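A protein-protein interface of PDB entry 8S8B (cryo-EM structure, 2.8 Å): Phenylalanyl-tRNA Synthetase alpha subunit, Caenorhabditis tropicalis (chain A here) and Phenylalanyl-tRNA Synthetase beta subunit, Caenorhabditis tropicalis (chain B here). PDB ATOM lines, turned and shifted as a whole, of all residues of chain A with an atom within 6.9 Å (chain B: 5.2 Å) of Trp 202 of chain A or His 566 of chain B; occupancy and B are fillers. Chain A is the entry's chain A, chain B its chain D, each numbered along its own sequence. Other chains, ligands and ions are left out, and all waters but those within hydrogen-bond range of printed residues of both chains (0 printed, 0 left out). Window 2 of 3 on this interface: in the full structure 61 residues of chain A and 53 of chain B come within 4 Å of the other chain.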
ATOM      1  N   LEU A 192       8.046  21.871  -2.518  1.00  0.00           N
ATOM      2  CA  LEU A 192       9.385  21.316  -2.627  1.00  0.00           C
ATOM      3  C   LEU A 192       9.427  20.339  -3.793  1.00  0.00           C
ATOM      4  O   LEU A 192       8.542  19.491  -3.930  1.00  0.00           O
ATOM      5  CB  LEU A 192       9.788  20.604  -1.336  1.00  0.00           C
ATOM      6  CG  LEU A 192       9.311  21.175   0.000  1.00  0.00           C
ATOM      7  CD1 LEU A 192       8.017  20.507   0.442  1.00  0.00           C
ATOM      8  CD2 LEU A 192      10.388  21.014   1.058  1.00  0.00           C
ATOM      9  N   MET A 196      14.693  18.237  -4.153  1.00  0.00           N
ATOM     10  CA  MET A 196      14.993  18.831  -2.854  1.00  0.00           C
ATOM     11  C   MET A 196      14.760  17.840  -1.721  1.00  0.00           C
ATOM     12  O   MET A 196      15.528  17.805  -0.753  1.00  0.00           O
ATOM     13  CB  MET A 196      14.162  20.097  -2.648  1.00  0.00           C
ATOM     14  CG  MET A 196      14.740  21.317  -3.340  1.00  0.00           C
ATOM     15  SD  MET A 196      13.971  22.861  -2.825  1.00  0.00           S
ATOM     16  CE  MET A 196      12.492  22.858  -3.824  1.00  0.00           C
ATOM     17  N   ILE A 197      13.704  17.031  -1.817  1.00  0.00           N
ATOM     18  CA  ILE A 197      13.450  16.021  -0.792  1.00  0.00           C
ATOM     19  C   ILE A 197      14.565  14.983  -0.781  1.00  0.00           C
ATOM     20  O   ILE A 197      15.036  14.565   0.283  1.00  0.00           O
ATOM     21  CB  ILE A 197      12.075  15.367  -1.009  1.00  0.00           C
ATOM     22  CG1 ILE A 197      10.960  16.400  -0.857  1.00  0.00           C
ATOM     23  CG2 ILE A 197      11.869  14.224  -0.033  1.00  0.00           C
ATOM     24  CD1 ILE A 197       9.574  15.821  -1.009  1.00  0.00           C
ATOM     25  N   ALA A 198      15.001  14.549  -1.965  1.00  0.00           N
ATOM     26  CA  ALA A 198      16.031  13.517  -2.038  1.00  0.00           C
ATOM     27  C   ALA A 198      17.377  14.034  -1.544  1.00  0.00           C
ATOM     28  O   ALA A 198      18.047  13.378  -0.738  1.00  0.00           O
ATOM     29  CB  ALA A 198      16.149  12.997  -3.470  1.00  0.00           C
ATOM     30  N   SER A 199      17.788  15.211  -2.012  1.00  0.00           N
ATOM     31  CA  SER A 199      19.105  15.748  -1.693  1.00  0.00           C
ATOM     32  C   SER A 199      19.143  16.520  -0.383  1.00  0.00           C
ATOM     33  O   SER A 199      20.236  16.870   0.074  1.00  0.00           O
ATOM     34  CB  SER A 199      19.589  16.654  -2.826  1.00  0.00           C
ATOM     35  OG  SER A 199      20.804  17.293  -2.478  1.00  0.00           O
ATOM     36  N   GLY A 200      17.997  16.795   0.227  1.00  0.00           N
ATOM     37  CA  GLY A 200      17.976  17.569   1.456  1.00  0.00           C
ATOM     38  C   GLY A 200      18.454  18.995   1.293  1.00  0.00           C
ATOM     39  O   GLY A 200      19.192  19.499   2.149  1.00  0.00           O
ATOM     40  N   SER A 201      18.053  19.661   0.211  1.00  0.00           N
ATOM     41  CA  SER A 201      18.433  21.041  -0.050  1.00  0.00           C
ATOM     42  C   SER A 201      17.345  22.028   0.354  1.00  0.00           C
ATOM     43  O   SER A 201      17.412  23.201  -0.023  1.00  0.00           O
ATOM     44  CB  SER A 201      18.781  21.223  -1.528  1.00  0.00           C
ATOM     45  OG  SER A 201      19.845  20.367  -1.909  1.00  0.00           O
ATOM     46  N   TRP A 202      16.349  21.578   1.116  1.00  0.00           N
ATOM     47  CA  TRP A 202      15.227  22.426   1.494  1.00  0.00           C
ATOM     48  C   TRP A 202      15.552  23.374   2.640  1.00  0.00           C
ATOM     49  O   TRP A 202      14.727  24.235   2.964  1.00  0.00           O
ATOM     50  CB  TRP A 202      14.028  21.559   1.875  1.00  0.00           C
ATOM     51  CG  TRP A 202      14.361  20.495   2.863  1.00  0.00           C
ATOM     52  CD1 TRP A 202      14.674  19.197   2.593  1.00  0.00           C
ATOM     53  CD2 TRP A 202      14.423  20.633   4.286  1.00  0.00           C
ATOM     54  NE1 TRP A 202      14.922  18.517   3.758  1.00  0.00           N
ATOM     55  CE2 TRP A 202      14.774  19.378   4.813  1.00  0.00           C
ATOM     56  CE3 TRP A 202      14.212  21.699   5.165  1.00  0.00           C
ATOM     57  CZ2 TRP A 202      14.919  19.156   6.179  1.00  0.00           C
ATOM     58  CZ3 TRP A 202      14.358  21.477   6.520  1.00  0.00           C
ATOM     59  CH2 TRP A 202      14.709  20.218   7.014  1.00  0.00           C
ATOM     60  N   LYS A 203      16.722  23.244   3.266  1.00  0.00           N
ATOM     61  CA  LYS A 203      17.080  24.064   4.417  1.00  0.00           C
ATOM     62  C   LYS A 203      18.087  25.156   4.073  1.00  0.00           C
ATOM     63  O   LYS A 203      18.746  25.690   4.972  1.00  0.00           O
ATOM     64  CB  LYS A 203      17.619  23.182   5.544  1.00  0.00           C
ATOM     65  CG  LYS A 203      18.830  22.356   5.158  1.00  0.00           C
ATOM     66  CD  LYS A 203      19.375  21.586   6.349  1.00  0.00           C
ATOM     67  CE  LYS A 203      18.374  20.561   6.847  1.00  0.00           C
ATOM     68  NZ  LYS A 203      18.123  19.508   5.829  1.00  0.00           N
ATOM     69  N   GLU A 204      18.223  25.505   2.793  1.00  0.00           N
ATOM     70  CA  GLU A 204      19.166  26.536   2.380  1.00  0.00           C
ATOM     71  C   GLU A 204      18.504  27.639   1.564  1.00  0.00           C
ATOM     72  O   GLU A 204      19.158  28.633   1.231  1.00  0.00           O
ATOM     73  CB  GLU A 204      20.315  25.920   1.575  1.00  0.00           C
ATOM     74  CG  GLU A 204      21.220  24.992   2.369  1.00  0.00           C
ATOM     75  CD  GLU A 204      20.654  23.593   2.504  1.00  0.00           C
ATOM     76  OE1 GLU A 204      19.512  23.364   2.054  1.00  0.00           O
ATOM     77  OE2 GLU A 204      21.355  22.720   3.058  1.00  0.00           O
ATOM     78  N   LYS A 205      17.226  27.487   1.233  1.00  0.00           N
ATOM     79  CA  LYS A 205      16.525  28.435   0.383  1.00  0.00           C
ATOM     80  C   LYS A 205      15.190  28.814   1.007  1.00  0.00           C
ATOM     81  O   LYS A 205      14.559  28.013   1.701  1.00  0.00           O
ATOM     82  CB  LYS A 205      16.313  27.855  -1.019  1.00  0.00           C
ATOM     83  CG  LYS A 205      15.723  26.457  -1.018  1.00  0.00           C
ATOM     84  CD  LYS A 205      15.903  25.783  -2.367  1.00  0.00           C
ATOM     85  CE  LYS A 205      17.373  25.594  -2.694  1.00  0.00           C
ATOM     86  NZ  LYS A 205      17.565  24.873  -3.980  1.00  0.00           N
ATOM     87  N   GLN A 206      14.767  30.049   0.750  1.00  0.00           N
ATOM     88  CA  GLN A 206      13.534  30.573   1.315  1.00  0.00           C
ATOM     89  C   GLN A 206      12.325  30.087   0.520  1.00  0.00           C
ATOM     90  O   GLN A 206      12.444  29.562  -0.589  1.00  0.00           O
ATOM     91  CB  GLN A 206      13.559  32.102   1.343  1.00  0.00           C
ATOM     92  CG  GLN A 206      14.664  32.707   2.195  1.00  0.00           C
ATOM     93  CD  GLN A 206      15.998  32.756   1.476  1.00  0.00           C
ATOM     94  OE1 GLN A 206      16.112  32.341   0.323  1.00  0.00           O
ATOM     95  NE2 GLN A 206      17.019  33.266   2.156  1.00  0.00           N
ATOM     96  N   PHE A 207      11.145  30.276   1.103  1.00  0.00           N
ATOM     97  CA  PHE A 207       9.894  29.895   0.469  1.00  0.00           C
ATOM     98  C   PHE A 207       8.912  31.059   0.516  1.00  0.00           C
ATOM     99  O   PHE A 207       9.023  31.964   1.346  1.00  0.00           O
ATOM    100  CB  PHE A 207       9.290  28.651   1.125  1.00  0.00           C
ATOM    101  CG  PHE A 207      10.020  27.386   0.787  1.00  0.00           C
ATOM    102  CD1 PHE A 207       9.721  26.690  -0.371  1.00  0.00           C
ATOM    103  CD2 PHE A 207      11.015  26.902   1.615  1.00  0.00           C
ATOM    104  CE1 PHE A 207      10.393  25.531  -0.692  1.00  0.00           C
ATOM    105  CE2 PHE A 207      11.690  25.741   1.299  1.00  0.00           C
ATOM    106  CZ  PHE A 207      11.378  25.055   0.144  1.00  0.00           C
ATOM    107  N   ARG B 428       7.904  13.464  14.157  1.00  0.00           N
ATOM    108  CA  ARG B 428       8.653  14.561  14.773  1.00  0.00           C
ATOM    109  C   ARG B 428       7.894  15.166  15.952  1.00  0.00           C
ATOM    110  O   ARG B 428       7.918  16.376  16.172  1.00  0.00           O
ATOM    111  CB  ARG B 428       9.004  15.634  13.743  1.00  0.00           C
ATOM    112  CG  ARG B 428       9.710  15.096  12.519  1.00  0.00           C
ATOM    113  CD  ARG B 428       9.991  16.188  11.505  1.00  0.00           C
ATOM    114  NE  ARG B 428      11.045  17.096  11.943  1.00  0.00           N
ATOM    115  CZ  ARG B 428      10.835  18.305  12.442  1.00  0.00           C
ATOM    116  NH1 ARG B 428       9.614  18.791  12.584  1.00  0.00           N
ATOM    117  NH2 ARG B 428      11.876  19.048  12.803  1.00  0.00           N
ATOM    118  N   PRO B 541       5.643  20.820  14.269  1.00  0.00           N
ATOM    119  CA  PRO B 541       6.809  20.079  13.764  1.00  0.00           C
ATOM    120  C   PRO B 541       6.502  19.158  12.597  1.00  0.00           C
ATOM    121  O   PRO B 541       7.359  18.984  11.723  1.00  0.00           O
ATOM    122  CB  PRO B 541       7.277  19.289  14.994  1.00  0.00           C
ATOM    123  CG  PRO B 541       6.694  20.011  16.162  1.00  0.00           C
ATOM    124  CD  PRO B 541       5.385  20.544  15.690  1.00  0.00           C
ATOM    125  N   THR B 542       5.311  18.558  12.550  1.00  0.00           N
ATOM    126  CA  THR B 542       5.010  17.576  11.516  1.00  0.00           C
ATOM    127  C   THR B 542       4.644  18.202  10.178  1.00  0.00           C
ATOM    128  O   THR B 542       4.530  17.474   9.187  1.00  0.00           O
ATOM    129  CB  THR B 542       3.875  16.653  11.966  1.00  0.00           C
ATOM    130  OG1 THR B 542       3.539  15.756  10.902  1.00  0.00           O
ATOM    131  CG2 THR B 542       2.652  17.455  12.337  1.00  0.00           C
ATOM    132  N   PHE B 543       4.457  19.516  10.119  1.00  0.00           N
ATOM    133  CA  PHE B 543       4.165  20.213   8.879  1.00  0.00           C
ATOM    134  C   PHE B 543       5.302  21.165   8.537  1.00  0.00           C
ATOM    135  O   PHE B 543       5.967  21.710   9.424  1.00  0.00           O
ATOM    136  CB  PHE B 543       2.849  20.989   8.972  1.00  0.00           C
ATOM    137  CG  PHE B 543       1.637  20.117   9.105  1.00  0.00           C
ATOM    138  CD1 PHE B 543       1.094  19.493   8.000  1.00  0.00           C
ATOM    139  CD2 PHE B 543       1.030  19.934  10.332  1.00  0.00           C
ATOM    140  CE1 PHE B 543      -0.021  18.695   8.118  1.00  0.00           C
ATOM    141  CE2 PHE B 543      -0.085  19.136  10.454  1.00  0.00           C
ATOM    142  CZ  PHE B 543      -0.611  18.517   9.346  1.00  0.00           C
ATOM    143  N   PHE B 544       5.520  21.356   7.243  1.00  0.00           N
ATOM    144  CA  PHE B 544       6.606  22.207   6.786  1.00  0.00           C
ATOM    145  C   PHE B 544       6.358  23.653   7.211  1.00  0.00           C
ATOM    146  O   PHE B 544       5.226  24.138   7.126  1.00  0.00           O
ATOM    147  CB  PHE B 544       6.739  22.114   5.268  1.00  0.00           C
ATOM    148  CG  PHE B 544       7.988  22.735   4.729  1.00  0.00           C
ATOM    149  CD1 PHE B 544       9.222  22.165   4.980  1.00  0.00           C
ATOM    150  CD2 PHE B 544       7.929  23.878   3.955  1.00  0.00           C
ATOM    151  CE1 PHE B 544      10.376  22.733   4.482  1.00  0.00           C
ATOM    152  CE2 PHE B 544       9.078  24.449   3.452  1.00  0.00           C
ATOM    153  CZ  PHE B 544      10.303  23.875   3.716  1.00  0.00           C
ATOM    154  N   PRO B 545       7.382  24.356   7.693  1.00  0.00           N
ATOM    155  CA  PRO B 545       7.187  25.749   8.113  1.00  0.00           C
ATOM    156  C   PRO B 545       6.721  26.623   6.959  1.00  0.00           C
ATOM    157  O   PRO B 545       7.198  26.503   5.829  1.00  0.00           O
ATOM    158  CB  PRO B 545       8.576  26.168   8.608  1.00  0.00           C
ATOM    159  CG  PRO B 545       9.254  24.893   8.957  1.00  0.00           C
ATOM    160  CD  PRO B 545       8.748  23.885   7.975  1.00  0.00           C
ATOM    161  N   ALA B 564       1.330  20.973   3.904  1.00  0.00           N
ATOM    162  CA  ALA B 564       2.340  20.082   3.353  1.00  0.00           C
ATOM    163  C   ALA B 564       3.189  19.476   4.462  1.00  0.00           C
ATOM    164  O   ALA B 564       3.532  20.137   5.444  1.00  0.00           O
ATOM    165  CB  ALA B 564       3.232  20.828   2.364  1.00  0.00           C
ATOM    166  N   LEU B 565       3.537  18.205   4.291  1.00  0.00           N
ATOM    167  CA  LEU B 565       4.291  17.488   5.306  1.00  0.00           C
ATOM    168  C   LEU B 565       5.780  17.800   5.198  1.00  0.00           C
ATOM    169  O   LEU B 565       6.290  18.185   4.144  1.00  0.00           O
ATOM    170  CB  LEU B 565       4.056  15.985   5.181  1.00  0.00           C
ATOM    171  CG  LEU B 565       2.598  15.537   5.271  1.00  0.00           C
ATOM    172  CD1 LEU B 565       2.502  14.026   5.205  1.00  0.00           C
ATOM    173  CD2 LEU B 565       1.960  16.054   6.541  1.00  0.00           C
ATOM    174  N   HIS B 566       6.477  17.628   6.318  1.00  0.00           N
ATOM    175  CA  HIS B 566       7.903  17.893   6.363  1.00  0.00           C
ATOM    176  C   HIS B 566       8.661  16.839   5.556  1.00  0.00           C
ATOM    177  O   HIS B 566       8.240  15.682   5.484  1.00  0.00           O
ATOM    178  CB  HIS B 566       8.392  17.897   7.810  1.00  0.00           C
ATOM    179  CG  HIS B 566       9.668  18.652   8.021  1.00  0.00           C
ATOM    180  ND1 HIS B 566      10.909  18.077   7.858  1.00  0.00           N
ATOM    181  CD2 HIS B 566       9.893  19.935   8.385  1.00  0.00           C
ATOM    182  CE1 HIS B 566      11.844  18.975   8.109  1.00  0.00           C
ATOM    183  NE2 HIS B 566      11.254  20.111   8.432  1.00  0.00           N
ATOM    184  N   PRO B 567       9.777  17.216   4.928  1.00  0.00           N
ATOM    185  CA  PRO B 567      10.561  16.220   4.181  1.00  0.00           C
ATOM    186  C   PRO B 567      11.027  15.050   5.027  1.00  0.00           C
ATOM    187  O   PRO B 567      11.087  13.920   4.526  1.00  0.00           O
ATOM    188  CB  PRO B 567      11.746  17.040   3.655  1.00  0.00           C
ATOM    189  CG  PRO B 567      11.223  18.421   3.561  1.00  0.00           C
ATOM    190  CD  PRO B 567      10.273  18.584   4.708  1.00  0.00           C
ATOM    191  N   GLU B 568      11.365  15.282   6.296  1.00  0.00           N
ATOM    192  CA  GLU B 568      11.779  14.182   7.160  1.00  0.00           C
ATOM    193  C   GLU B 568      10.640  13.204   7.409  1.00  0.00           C
ATOM    194  O   GLU B 568      10.862  11.988   7.431  1.00  0.00           O
ATOM    195  CB  GLU B 568      12.320  14.730   8.477  1.00  0.00           C
ATOM    196  CG  GLU B 568      13.527  15.634   8.299  1.00  0.00           C
ATOM    197  CD  GLU B 568      14.096  16.117   9.613  1.00  0.00           C
ATOM    198  OE1 GLU B 568      13.583  15.703  10.673  1.00  0.00           O
ATOM    199  OE2 GLU B 568      15.059  16.911   9.588  1.00  0.00           O
ATOM    200  N   VAL B 569       9.417  13.708   7.586  1.00  0.00           N
ATOM    201  CA  VAL B 569       8.267  12.825   7.743  1.00  0.00           C
ATOM    202  C   VAL B 569       8.052  12.005   6.478  1.00  0.00           C
ATOM    203  O   VAL B 569       7.662  10.833   6.540  1.00  0.00           O
ATOM    204  CB  VAL B 569       7.013  13.636   8.108  1.00  0.00           C
ATOM    205  CG1 VAL B 569       5.850  12.708   8.414  1.00  0.00           C
ATOM    206  CG2 VAL B 569       7.298  14.544   9.285  1.00  0.00           C
ATOM    207  N   ILE B 570       8.289  12.609   5.313  1.00  0.00           N
ATOM    208  CA  ILE B 570       8.155  11.879   4.057  1.00  0.00           C
ATOM    209  C   ILE B 570       9.190  10.766   3.972  1.00  0.00           C
ATOM    210  O   ILE B 570       8.864   9.616   3.658  1.00  0.00           O
ATOM    211  CB  ILE B 570       8.270  12.845   2.863  1.00  0.00           C
ATOM    212  CG1 ILE B 570       7.009  13.697   2.741  1.00  0.00           C
ATOM    213  CG2 ILE B 570       8.533  12.082   1.578  1.00  0.00           C
ATOM    214  CD1 ILE B 570       7.073  14.709   1.624  1.00  0.00           C
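His 566 of chain B touches one residue of chain A.
Printed residues of chain B within 4 Å of Ile 197 of chain A: Ile 570.
Of the printed residues of chain A, Phe 544 of chain B touches Leu 192 (3.8 Å) and Phe 207 (3.4 Å).
Of the printed residues of chain B, Phe 207 of chain A touches Phe 544.
Printed residues of chain A within 4 Å of Ile 570 of chain B: Ile 197.
Pro 545 of chain B touches none of the printed residues of chain A.
The nearest residue of chain B that does not touch Trp 202 of chain A is Phe 544 of chain B (4.03 Å).
The nearest residue of chain A that does not touch His 566 of chain B is Leu 192 of chain A (6.3 Å).
Hydrophobic or aromatic side chains of chain B that line the printed part of chain A: Phe 544, His 566, Pro 567 and Ile 570.
Along chain B the printed residues that touch a printed residue of chain A span positions 544 to 570.
Of the 13 printed residues of chain A, 4 touch a printed residue of chain B.
Among the printed residues, 6 pairs touch across the chains.
Among the printed residues, no Asp or Glu carboxylate lies within 4 Å of a Lys or Arg side-chain nitrogen of the other chain.
Among the printed residues, pairs that only touch across the chains: Trp 202 of chain A with His 566 of chain B (3.3 Å), Phe 207 of chain A with Phe 544 of chain B (3.4 Å), Trp 202 of chain A with Pro 567 of chain B (3.5 Å), Leu 192 of chain A with Pro 567 of chain B (3.7 Å), Ile 197 of chain A with Ile 570 of chain B (3.8 Å) and Leu 192 of chain A with Phe 544 of chain B (3.8 Å).
The backbone NH (N) of His 566 of chain B sits at hydrogen-bond distance from the backbone carbonyl oxygen (O) of Thr 542 of chain B, at 3.5 Å.
N of Glu 568 of chain B sits close to ND1 of His 566 of chain B (3.2 Å).
N of Phe 544 of chain B is in hydrogen-bond range of O of Ala 564 of chain B (2.9 Å).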
